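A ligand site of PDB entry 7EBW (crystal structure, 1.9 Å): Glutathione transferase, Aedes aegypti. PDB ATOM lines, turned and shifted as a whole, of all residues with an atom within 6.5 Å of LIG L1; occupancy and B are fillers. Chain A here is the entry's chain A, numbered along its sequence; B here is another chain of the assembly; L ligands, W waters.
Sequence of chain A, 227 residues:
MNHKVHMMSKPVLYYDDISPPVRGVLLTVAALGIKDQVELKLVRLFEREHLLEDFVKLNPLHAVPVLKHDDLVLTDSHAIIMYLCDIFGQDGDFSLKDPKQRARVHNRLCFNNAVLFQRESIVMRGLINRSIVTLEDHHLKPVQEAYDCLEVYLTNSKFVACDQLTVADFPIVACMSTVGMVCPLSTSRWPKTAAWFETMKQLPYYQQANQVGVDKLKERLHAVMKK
The side-chain hydroxyl (OG) of Ser 19 lies within hydrogen-bond range of the backbone NH (N) of Val 22 (3.3 Å).
The backbone carbonyl oxygen (O) of Asn 113 sits at hydrogen-bond distance from the side-chain amide nitrogen (NE2) of Gln 118 (2.8 Å).
The backbone carbonyl oxygen (O) of Asn 112 sits at hydrogen-bond distance from the backbone NH (N) of Phe 117, 2.8 Å away.
The backbone carbonyl oxygen of Phe 117 sits at hydrogen-bond distance from the side-chain hydroxyl of Ser 121, 3.0 Å away.
OD2 of Asp 76 is in hydrogen-bond range of ND2 of Asn 113.
OD1 of Asp 76 is in hydrogen-bond range of ND1 of His 78 (2.8 Å).
OG of Ser 77 is in hydrogen-bond range of ND1 of His 78, 3.2 Å away.
A ring nitrogen (NE2) of His 78 is in hydrogen-bond range of the side-chain amide nitrogen (ND2) of Asn 112.
Water W3 bridges an oxygen (O6) of LIG L1 (2.7 Å) and a ring nitrogen (NE2) of His 50 (3.0 Å).
Water W6 lies within hydrogen-bond range of O of Pro 65 (2.7 Å), O2 of LIG L1 (2.9 Å) and O of Val 64 (3.4 Å).
Water W2 lies within hydrogen-bond range of a nitrogen (N1) of LIG L1, the side-chain amide nitrogen of Gln 118 and the backbone carbonyl oxygen of Ala 114 of chain B.
Water W1 lies within hydrogen-bond range of the guanidinium group (NH1) of Arg 125 (2.7 Å), an oxygen (O5) of LG2 L2 (2.8 Å) and a nitrogen (N3) of LIG L1 (2.9 Å).
Residues that only touch LIG L1: Ala 63, Pro 65, His 50, Phe 117, Pro 21, Leu 45, Ala 114 of chain B and Pro 20.
Hydrophobic or aromatic side chains within 4 Å of LIG L1: Pro 20, Pro 21, Leu 45, His 50, His 62, Ala 63, Val 64, Pro 65, His 78, Phe 117 and Ala 114 of chain B.
The nearest printed residue that does not touch LIG L1 is Thr 75 (4.5 Å).
A ring nitrogen (ND1) of His 78 sits at hydrogen-bond distance from an oxygen (O1) of LIG L1 (3.4 Å).
OE2 of Glu 120 sits at hydrogen-bond distance from O2 of LG2 L2 (2.5 Å).
O of Leu 45 is in hydrogen-bond range of O4 of LG2 L2 (3.3 Å).
O of Val 64 is in hydrogen-bond range of N2 of LIG L1 (3.0 Å).
OD1 of Asn 113 sits at hydrogen-bond distance from N1 of LIG L1, 2.9 Å away.
OD2 of Asp 76 is in salt-bridge range of N1 of LIG L1 (2.9 Å).
N of Val 64 lies within hydrogen-bond range of O4 of LIG L1 (2.9 Å).
The backbone NH of Ser 77 sits at hydrogen-bond distance from an oxygen (O2) of LIG L1 (2.7 Å).
A ring nitrogen (ND1) of His 62 is in hydrogen-bond range of an oxygen (O6) of LIG L1, 2.9 Å away.
O5 of LIG L1 lies within salt-bridge range of NH1 of Arg 125.
The side-chain hydroxyl (OG) of Ser 77 is in hydrogen-bond range of an oxygen (O1) of LIG L1.
S1 of LIG L1 lies close to OG of Ser 19 (3.3 Å).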
ATOM      1  N   ILE A  18      14.640 -14.442  22.329  1.00  0.00           N
ATOM      2  CA  ILE A  18      15.623 -14.749  21.292  1.00  0.00           C
ATOM      3  C   ILE A  18      15.377 -13.951  20.011  1.00  0.00           C
ATOM      4  O   ILE A  18      16.306 -13.726  19.232  1.00  0.00           O
ATOM      5  CB  ILE A  18      15.625 -16.279  21.144  1.00  0.00           C
ATOM      6  CG1 ILE A  18      14.353 -16.785  20.457  1.00  0.00           C
ATOM      7  CG2 ILE A  18      15.901 -16.968  22.484  1.00  0.00           C
ATOM      8  CD1 ILE A  18      14.603 -17.916  19.545  1.00  0.00           C
ATOM      9  N   SER A  19      14.144 -13.465  19.823  1.00  0.00           N
ATOM     10  CA  SER A  19      13.736 -12.700  18.648  1.00  0.00           C
ATOM     11  C   SER A  19      14.219 -11.257  18.751  1.00  0.00           C
ATOM     12  O   SER A  19      13.888 -10.582  19.734  1.00  0.00           O
ATOM     13  CB  SER A  19      12.216 -12.739  18.527  1.00  0.00           C
ATOM     14  OG  SER A  19      11.710 -11.730  17.676  1.00  0.00           O
ATOM     15  N   PRO A  20      14.992 -10.737  17.783  1.00  0.00           N
ATOM     16  CA  PRO A  20      15.361  -9.307  17.796  1.00  0.00           C
ATOM     17  C   PRO A  20      14.143  -8.389  17.836  1.00  0.00           C
ATOM     18  O   PRO A  20      14.119  -7.442  18.639  1.00  0.00           O
ATOM     19  CB  PRO A  20      16.141  -9.132  16.477  1.00  0.00           C
ATOM     20  CG  PRO A  20      16.617 -10.473  16.134  1.00  0.00           C
ATOM     21  CD  PRO A  20      15.586 -11.451  16.650  1.00  0.00           C
ATOM     22  N   PRO A  21      13.101  -8.610  17.011  1.00  0.00           N
ATOM     23  CA  PRO A  21      11.906  -7.760  17.142  1.00  0.00           C
ATOM     24  C   PRO A  21      11.349  -7.717  18.554  1.00  0.00           C
ATOM     25  O   PRO A  21      10.970  -6.638  19.042  1.00  0.00           O
ATOM     26  CB  PRO A  21      10.904  -8.404  16.164  1.00  0.00           C
ATOM     27  CG  PRO A  21      11.744  -8.995  15.129  1.00  0.00           C
ATOM     28  CD  PRO A  21      12.959  -9.522  15.863  1.00  0.00           C
ATOM     29  N   VAL A  22      11.297  -8.862  19.228  1.00  0.00           N
ATOM     30  CA  VAL A  22      10.877  -8.873  20.625  1.00  0.00           C
ATOM     31  C   VAL A  22      11.798  -7.992  21.465  1.00  0.00           C
ATOM     32  O   VAL A  22      11.337  -7.193  22.281  1.00  0.00           O
ATOM     33  CB  VAL A  22      10.824 -10.315  21.163  1.00  0.00           C
ATOM     34  CG1 VAL A  22      10.779 -10.294  22.693  1.00  0.00           C
ATOM     35  CG2 VAL A  22       9.589 -11.085  20.575  1.00  0.00           C
ATOM     36  N   LEU A  45       9.389 -20.047  20.647  1.00  0.00           N
ATOM     37  CA  LEU A  45       9.466 -20.381  19.226  1.00  0.00           C
ATOM     38  C   LEU A  45       9.980 -21.794  19.007  1.00  0.00           C
ATOM     39  O   LEU A  45       9.436 -22.540  18.193  1.00  0.00           O
ATOM     40  CB  LEU A  45      10.360 -19.367  18.512  1.00  0.00           C
ATOM     41  CG  LEU A  45       9.752 -17.956  18.474  1.00  0.00           C
ATOM     42  CD1 LEU A  45      10.734 -16.944  17.852  1.00  0.00           C
ATOM     43  CD2 LEU A  45       8.486 -18.040  17.676  1.00  0.00           C
ATOM     44  N   HIS A  50       4.100 -20.778  19.006  1.00  0.00           N
ATOM     45  CA  HIS A  50       3.502 -19.794  18.100  1.00  0.00           C
ATOM     46  C   HIS A  50       2.612 -20.436  17.060  1.00  0.00           C
ATOM     47  O   HIS A  50       1.938 -19.720  16.315  1.00  0.00           O
ATOM     48  CB  HIS A  50       4.598 -18.975  17.412  1.00  0.00           C
ATOM     49  CG  HIS A  50       5.549 -19.806  16.601  1.00  0.00           C
ATOM     50  ND1 HIS A  50       6.347 -20.777  17.172  1.00  0.00           N
ATOM     51  CD2 HIS A  50       5.854 -19.794  15.285  1.00  0.00           C
ATOM     52  CE1 HIS A  50       7.081 -21.359  16.228  1.00  0.00           C
ATOM     53  NE2 HIS A  50       6.797 -20.776  15.078  1.00  0.00           N
ATOM     54  N   LEU A  51       2.590 -21.767  16.976  1.00  0.00           N
ATOM     55  CA  LEU A  51       1.740 -22.466  16.026  1.00  0.00           C
ATOM     56  C   LEU A  51       0.484 -23.009  16.673  1.00  0.00           C
ATOM     57  O   LEU A  51      -0.341 -23.613  15.982  1.00  0.00           O
ATOM     58  CB  LEU A  51       2.531 -23.599  15.355  1.00  0.00           C
ATOM     59  CG  LEU A  51       3.805 -23.111  14.650  1.00  0.00           C
ATOM     60  CD1 LEU A  51       4.622 -24.265  14.017  1.00  0.00           C
ATOM     61  CD2 LEU A  51       3.433 -22.107  13.586  1.00  0.00           C
ATOM     62  N   LEU A  61       0.010 -14.340  11.314  1.00  0.00           N
ATOM     63  CA  LEU A  61       1.423 -14.396  10.941  1.00  0.00           C
ATOM     64  C   LEU A  61       2.215 -15.352  11.818  1.00  0.00           C
ATOM     65  O   LEU A  61       3.380 -15.630  11.505  1.00  0.00           O
ATOM     66  CB  LEU A  61       2.023 -12.975  11.010  1.00  0.00           C
ATOM     67  CG  LEU A  61       1.454 -11.952  10.015  1.00  0.00           C
ATOM     68  CD1 LEU A  61       1.812 -10.512  10.406  1.00  0.00           C
ATOM     69  CD2 LEU A  61       1.940 -12.263   8.588  1.00  0.00           C
ATOM     70  N   HIS A  62       1.618 -15.863  12.895  1.00  0.00           N
ATOM     71  CA  HIS A  62       2.261 -16.804  13.805  1.00  0.00           C
ATOM     72  C   HIS A  62       3.699 -16.384  14.147  1.00  0.00           C
ATOM     73  O   HIS A  62       4.660 -17.139  14.010  1.00  0.00           O
ATOM     74  CB  HIS A  62       2.202 -18.244  13.278  1.00  0.00           C
ATOM     75  CG  HIS A  62       2.669 -18.427  11.870  1.00  0.00           C
ATOM     76  ND1 HIS A  62       3.996 -18.646  11.538  1.00  0.00           N
ATOM     77  CD2 HIS A  62       1.985 -18.457  10.693  1.00  0.00           C
ATOM     78  CE1 HIS A  62       4.108 -18.778  10.227  1.00  0.00           C
ATOM     79  NE2 HIS A  62       2.902 -18.671   9.699  1.00  0.00           N
ATOM     80  N   ALA A  63       3.833 -15.130  14.591  1.00  0.00           N
ATOM     81  CA  ALA A  63       5.141 -14.576  14.919  1.00  0.00           C
ATOM     82  C   ALA A  63       5.051 -13.737  16.185  1.00  0.00           C
ATOM     83  O   ALA A  63       3.990 -13.238  16.569  1.00  0.00           O
ATOM     84  CB  ALA A  63       5.690 -13.745  13.750  1.00  0.00           C
ATOM     85  N   VAL A  64       6.204 -13.594  16.844  1.00  0.00           N
ATOM     86  CA  VAL A  64       6.337 -12.741  18.016  1.00  0.00           C
ATOM     87  C   VAL A  64       7.205 -11.544  17.638  1.00  0.00           C
ATOM     88  O   VAL A  64       8.145 -11.685  16.835  1.00  0.00           O
ATOM     89  CB  VAL A  64       6.923 -13.508  19.220  1.00  0.00           C
ATOM     90  CG1 VAL A  64       5.929 -14.605  19.706  1.00  0.00           C
ATOM     91  CG2 VAL A  64       8.288 -14.134  18.876  1.00  0.00           C
ATOM     92  N   PRO A  65       6.975 -10.355  18.218  1.00  0.00           N
ATOM     93  CA  PRO A  65       6.009 -10.130  19.308  1.00  0.00           C
ATOM     94  C   PRO A  65       4.573  -9.830  18.886  1.00  0.00           C
ATOM     95  O   PRO A  65       4.295  -9.446  17.753  1.00  0.00           O
ATOM     96  CB  PRO A  65       6.572  -8.904  20.019  1.00  0.00           C
ATOM     97  CG  PRO A  65       7.201  -8.123  18.881  1.00  0.00           C
ATOM     98  CD  PRO A  65       7.761  -9.153  17.903  1.00  0.00           C
ATOM     99  N   THR A  75       0.603  -6.677  15.790  1.00  0.00           N
ATOM    100  CA  THR A  75       1.298  -7.885  15.354  1.00  0.00           C
ATOM    101  C   THR A  75       2.591  -7.522  14.641  1.00  0.00           C
ATOM    102  O   THR A  75       3.016  -8.193  13.718  1.00  0.00           O
ATOM    103  CB  THR A  75       0.405  -8.737  14.469  1.00  0.00           C
ATOM    104  OG1 THR A  75      -0.076  -7.942  13.382  1.00  0.00           O
ATOM    105  CG2 THR A  75      -0.790  -9.253  15.280  1.00  0.00           C
ATOM    106  N   ASP A  76       3.242  -6.459  15.111  1.00  0.00           N
ATOM    107  CA  ASP A  76       4.554  -6.075  14.591  1.00  0.00           C
ATOM    108  C   ASP A  76       5.254  -5.274  15.666  1.00  0.00           C
ATOM    109  O   ASP A  76       4.673  -4.323  16.185  1.00  0.00           O
ATOM    110  CB  ASP A  76       4.437  -5.255  13.317  1.00  0.00           C
ATOM    111  CG  ASP A  76       5.770  -5.112  12.599  1.00  0.00           C
ATOM    112  OD1 ASP A  76       6.646  -4.411  13.137  1.00  0.00           O
ATOM    113  OD2 ASP A  76       5.952  -5.723  11.534  1.00  0.00           O
ATOM    114  N   SER A  77       6.476  -5.671  16.007  1.00  0.00           N
ATOM    115  CA  SER A  77       7.254  -4.982  17.034  1.00  0.00           C
ATOM    116  C   SER A  77       7.285  -3.477  16.830  1.00  0.00           C
ATOM    117  O   SER A  77       7.262  -2.713  17.791  1.00  0.00           O
ATOM    118  CB  SER A  77       8.678  -5.543  17.063  1.00  0.00           C
ATOM    119  OG  SER A  77       9.368  -5.192  15.869  1.00  0.00           O
ATOM    120  N   HIS A  78       7.345  -3.043  15.564  1.00  0.00           N
ATOM    121  CA  HIS A  78       7.530  -1.623  15.282  1.00  0.00           C
ATOM    122  C   HIS A  78       6.280  -0.822  15.605  1.00  0.00           C
ATOM    123  O   HIS A  78       6.372   0.279  16.155  1.00  0.00           O
ATOM    124  CB  HIS A  78       7.981  -1.440  13.825  1.00  0.00           C
ATOM    125  CG  HIS A  78       9.265  -2.160  13.537  1.00  0.00           C
ATOM    126  ND1 HIS A  78       9.302  -3.478  13.135  1.00  0.00           N
ATOM    127  CD2 HIS A  78      10.554  -1.779  13.697  1.00  0.00           C
ATOM    128  CE1 HIS A  78      10.563  -3.861  13.001  1.00  0.00           C
ATOM    129  NE2 HIS A  78      11.341  -2.844  13.339  1.00  0.00           N
ATOM    130  N   ILE A  80       4.083  -1.943  17.858  1.00  0.00           N
ATOM    131  CA  ILE A  80       4.009  -2.034  19.319  1.00  0.00           C
ATOM    132  C   ILE A  80       4.835  -0.917  19.969  1.00  0.00           C
ATOM    133  O   ILE A  80       4.397  -0.296  20.955  1.00  0.00           O
ATOM    134  CB  ILE A  80       4.476  -3.431  19.775  1.00  0.00           C
ATOM    135  CG1 ILE A  80       3.501  -4.505  19.254  1.00  0.00           C
ATOM    136  CG2 ILE A  80       4.675  -3.463  21.311  1.00  0.00           C
ATOM    137  CD1 ILE A  80       4.019  -5.970  19.421  1.00  0.00           C
ATOM    138  N   ASN A 112      14.527  -0.477   9.934  1.00  0.00           N
ATOM    139  CA  ASN A 112      14.808  -1.745  10.598  1.00  0.00           C
ATOM    140  C   ASN A 112      13.867  -2.834  10.116  1.00  0.00           C
ATOM    141  O   ASN A 112      14.307  -3.927   9.741  1.00  0.00           O
ATOM    142  CB  ASN A 112      14.707  -1.613  12.127  1.00  0.00           C
ATOM    143  CG  ASN A 112      15.161  -2.894  12.832  1.00  0.00           C
ATOM    144  OD1 ASN A 112      16.351  -3.229  12.803  1.00  0.00           O
ATOM    145  ND2 ASN A 112      14.218  -3.644  13.435  1.00  0.00           N
ATOM    146  N   ASN A 113      12.569  -2.538  10.081  1.00  0.00           N
ATOM    147  CA  ASN A 113      11.581  -3.542   9.697  1.00  0.00           C
ATOM    148  C   ASN A 113      11.804  -4.019   8.264  1.00  0.00           C
ATOM    149  O   ASN A 113      11.757  -5.228   7.992  1.00  0.00           O
ATOM    150  CB  ASN A 113      10.170  -2.971   9.833  1.00  0.00           C
ATOM    151  CG  ASN A 113       9.149  -4.059  10.128  1.00  0.00           C
ATOM    152  OD1 ASN A 113       9.520  -5.177  10.455  1.00  0.00           O
ATOM    153  ND2 ASN A 113       7.881  -3.718  10.055  1.00  0.00           N
ATOM    154  N   PHE A 117      16.329  -5.831   9.490  1.00  0.00           N
ATOM    155  CA  PHE A 117      15.793  -7.080  10.017  1.00  0.00           C
ATOM    156  C   PHE A 117      15.447  -8.040   8.891  1.00  0.00           C
ATOM    157  O   PHE A 117      15.612  -9.255   9.045  1.00  0.00           O
ATOM    158  CB  PHE A 117      14.568  -6.848  10.904  1.00  0.00           C
ATOM    159  CG  PHE A 117      13.872  -8.136  11.269  1.00  0.00           C
ATOM    160  CD1 PHE A 117      14.480  -9.022  12.152  1.00  0.00           C
ATOM    161  CD2 PHE A 117      12.646  -8.479  10.703  1.00  0.00           C
ATOM    162  CE1 PHE A 117      13.885 -10.209  12.482  1.00  0.00           C
ATOM    163  CE2 PHE A 117      12.047  -9.677  11.045  1.00  0.00           C
ATOM    164  CZ  PHE A 117      12.672 -10.551  11.938  1.00  0.00           C
ATOM    165  N   GLN A 118      14.945  -7.540   7.760  1.00  0.00           N
ATOM    166  CA  GLN A 118      14.660  -8.446   6.647  1.00  0.00           C
ATOM    167  C   GLN A 118      15.910  -9.196   6.250  1.00  0.00           C
ATOM    168  O   GLN A 118      15.877 -10.421   6.056  1.00  0.00           O
ATOM    169  CB  GLN A 118      14.088  -7.682   5.446  1.00  0.00           C
ATOM    170  CG  GLN A 118      12.667  -7.126   5.677  1.00  0.00           C
ATOM    171  CD  GLN A 118      11.680  -8.173   6.234  1.00  0.00           C
ATOM    172  OE1 GLN A 118      11.609  -9.303   5.745  1.00  0.00           O
ATOM    173  NE2 GLN A 118      10.914  -7.781   7.263  1.00  0.00           N
ATOM    174  N   GLU A 120      18.740  -9.610   8.077  1.00  0.00           N
ATOM    175  CA  GLU A 120      19.145 -10.474   9.173  1.00  0.00           C
ATOM    176  C   GLU A 120      18.336 -11.757   9.184  1.00  0.00           C
ATOM    177  O   GLU A 120      18.890 -12.856   9.400  1.00  0.00           O
ATOM    178  CB  GLU A 120      19.016  -9.735  10.511  1.00  0.00           C
ATOM    179  CG  GLU A 120      19.433 -10.528  11.777  1.00  0.00           C
ATOM    180  CD  GLU A 120      18.380 -11.444  12.379  1.00  0.00           C
ATOM    181  OE1 GLU A 120      17.174 -11.298  12.100  1.00  0.00           O
ATOM    182  OE2 GLU A 120      18.775 -12.314  13.154  1.00  0.00           O
ATOM    183  N   SER A 121      17.033 -11.662   8.939  1.00  0.00           N
ATOM    184  CA  SER A 121      16.168 -12.822   9.112  1.00  0.00           C
ATOM    185  C   SER A 121      16.340 -13.843   8.000  1.00  0.00           C
ATOM    186  O   SER A 121      16.222 -15.048   8.248  1.00  0.00           O
ATOM    187  CB  SER A 121      14.703 -12.396   9.205  1.00  0.00           C
ATOM    188  OG  SER A 121      14.305 -11.764   8.011  1.00  0.00           O
ATOM    189  N   ARG A 125      17.128 -17.261   9.646  1.00  0.00           N
ATOM    190  CA  ARG A 125      16.147 -18.322   9.421  1.00  0.00           C
ATOM    191  C   ARG A 125      16.759 -19.478   8.644  1.00  0.00           C
ATOM    192  O   ARG A 125      16.516 -20.648   8.944  1.00  0.00           O
ATOM    193  CB  ARG A 125      14.936 -17.764   8.661  1.00  0.00           C
ATOM    194  CG  ARG A 125      13.785 -17.274   9.524  1.00  0.00           C
ATOM    195  CD  ARG A 125      12.749 -16.510   8.679  1.00  0.00           C
ATOM    196  NE  ARG A 125      11.855 -17.354   7.905  1.00  0.00           N
ATOM    197  CZ  ARG A 125      10.721 -17.881   8.353  1.00  0.00           C
ATOM    198  NH1 ARG A 125      10.333 -17.705   9.615  1.00  0.00           N
ATOM    199  NH2 ARG A 125       9.955 -18.573   7.534  1.00  0.00           N
ATOM    200  N   CYS B 110       2.826  -1.899   8.660  1.00  0.00           N
ATOM    201  CA  CYS B 110       3.921  -2.822   8.939  1.00  0.00           C
ATOM    202  C   CYS B 110       3.716  -4.134   8.212  1.00  0.00           C
ATOM    203  O   CYS B 110       4.671  -4.702   7.658  1.00  0.00           O
ATOM    204  CB  CYS B 110       4.033  -3.078  10.438  1.00  0.00           C
ATOM    205  SG  CYS B 110       4.602  -1.652  11.391  1.00  0.00           S
ATOM    206  N   ALA B 114       6.592  -5.173   5.751  1.00  0.00           N
ATOM    207  CA  ALA B 114       7.439  -6.271   6.203  1.00  0.00           C
ATOM    208  C   ALA B 114       7.053  -7.638   5.667  1.00  0.00           C
ATOM    209  O   ALA B 114       7.869  -8.564   5.712  1.00  0.00           O
ATOM    210  CB  ALA B 114       7.448  -6.337   7.738  1.00  0.00           C
ATOM    211  N   VAL B 115       5.831  -7.791   5.159  1.00  0.00           N
ATOM    212  CA  VAL B 115       5.366  -9.115   4.729  1.00  0.00           C
ATOM    213  C   VAL B 115       4.962  -9.069   3.262  1.00  0.00           C
ATOM    214  O   VAL B 115       5.626  -9.664   2.417  1.00  0.00           O
ATOM    215  CB  VAL B 115       4.210  -9.591   5.628  1.00  0.00           C
ATOM    216  CG1 VAL B 115       3.714 -10.962   5.185  1.00  0.00           C
ATOM    217  CG2 VAL B 115       4.658  -9.632   7.098  1.00  0.00           C
HETATM  218  N1  LIG L   1       8.180  -7.556  11.329  1.00  0.00           N
HETATM  219  C1  LIG L   1       7.871  -8.416  12.508  1.00  0.00           C
HETATM  220  C2  LIG L   1       8.095  -7.626  13.807  1.00  0.00           C
HETATM  221  O1  LIG L   1       8.978  -6.750  13.787  1.00  0.00           O
HETATM  222  O2  LIG L   1       7.374  -7.923  14.799  1.00  0.00           O
HETATM  223  C3  LIG L   1       8.728  -9.686  12.454  1.00  0.00           C
HETATM  224  C4  LIG L   1       8.391 -10.718  13.527  1.00  0.00           C
HETATM  225  C5  LIG L   1       9.189 -11.983  13.291  1.00  0.00           C
HETATM  226  O3  LIG L   1       9.681 -12.239  12.192  1.00  0.00           O
HETATM  227  N2  LIG L   1       9.327 -12.795  14.347  1.00  0.00           N
HETATM  228  C6  LIG L   1       9.916 -14.110  14.257  1.00  0.00           C
HETATM  229  C7  LIG L   1       8.945 -15.267  14.460  1.00  0.00           C
HETATM  230  O4  LIG L   1       8.171 -15.230  15.418  1.00  0.00           O
HETATM  231  C8  LIG L   1      11.059 -14.250  15.252  1.00  0.00           C
HETATM  232  S1  LIG L   1      12.464 -13.181  14.865  1.00  0.00           S
HETATM  233  N3  LIG L   1       8.994 -16.259  13.578  1.00  0.00           N
HETATM  234  C9  LIG L   1       8.121 -17.416  13.656  1.00  0.00           C
HETATM  235  C10 LIG L   1       7.483 -17.726  12.303  1.00  0.00           C
HETATM  236  O5  LIG L   1       7.739 -16.934  11.373  1.00  0.00           O
HETATM  237  O6  LIG L   1       6.776 -18.743  12.220  1.00  0.00           O
HETATM  238  C1  LG2 L   2      15.119 -16.247  15.423  1.00  0.00           C
HETATM  239  C2  LG2 L   2      14.531 -16.497  14.164  1.00  0.00           C
HETATM  240  C3  LG2 L   2      13.623 -17.635  13.976  1.00  0.00           C
HETATM  241  C4  LG2 L   2      13.355 -18.491  15.085  1.00  0.00           C
HETATM  242  C5  LG2 L   2      13.974 -18.229  16.396  1.00  0.00           C
HETATM  243  O1  LG2 L   2      14.885 -17.111  16.631  1.00  0.00           O
HETATM  244  C6  LG2 L   2      15.972 -15.170  15.641  1.00  0.00           C
HETATM  245  C7  LG2 L   2      16.260 -14.325  14.577  1.00  0.00           C
HETATM  246  C8  LG2 L   2      15.670 -14.534  13.298  1.00  0.00           C
HETATM  247  C9  LG2 L   2      14.813 -15.624  13.083  1.00  0.00           C
HETATM  248  O2  LG2 L   2      17.135 -13.280  14.847  1.00  0.00           O
HETATM  249  O3  LG2 L   2      15.946 -13.670  12.239  1.00  0.00           O
HETATM  250  C10 LG2 L   2      12.449 -19.717  15.043  1.00  0.00           C
HETATM  251  C11 LG2 L   2      12.864 -20.880  15.695  1.00  0.00           C
HETATM  252  C12 LG2 L   2      12.065 -22.010  15.670  1.00  0.00           C
HETATM  253  C13 LG2 L   2      10.826 -21.955  15.038  1.00  0.00           C
HETATM  254  C14 LG2 L   2      10.399 -20.787  14.425  1.00  0.00           C
HETATM  255  C15 LG2 L   2      11.207 -19.673  14.423  1.00  0.00           C
HETATM  256  O4  LG2 L   2      10.004 -23.085  15.022  1.00  0.00           O
HETATM  257  O5  LG2 L   2      13.124 -17.844  12.912  1.00  0.00           O
HETATM  258  O   HOH W   1      11.208 -16.231  11.662  1.00  0.00           O
HETATM  259  O   HOH W   2       8.724  -9.240   9.029  1.00  0.00           O
HETATM  260  O   HOH W   3       7.414 -21.376  12.225  1.00  0.00           O
HETATM  261  O   HOH W   4       8.391 -14.412  10.665  1.00  0.00           O
HETATM  262  O   HOH W   5       7.002 -16.753   8.590  1.00  0.00           O
HETATM  263  O   HOH W   6       5.556 -10.060  15.412  1.00  0.00           O
HETATM  264  O   HOH W   7      12.038 -13.958  11.011  1.00  0.00           O
HETATM  265  O   HOH W   8       9.327 -11.766   9.418  1.00  0.00           O
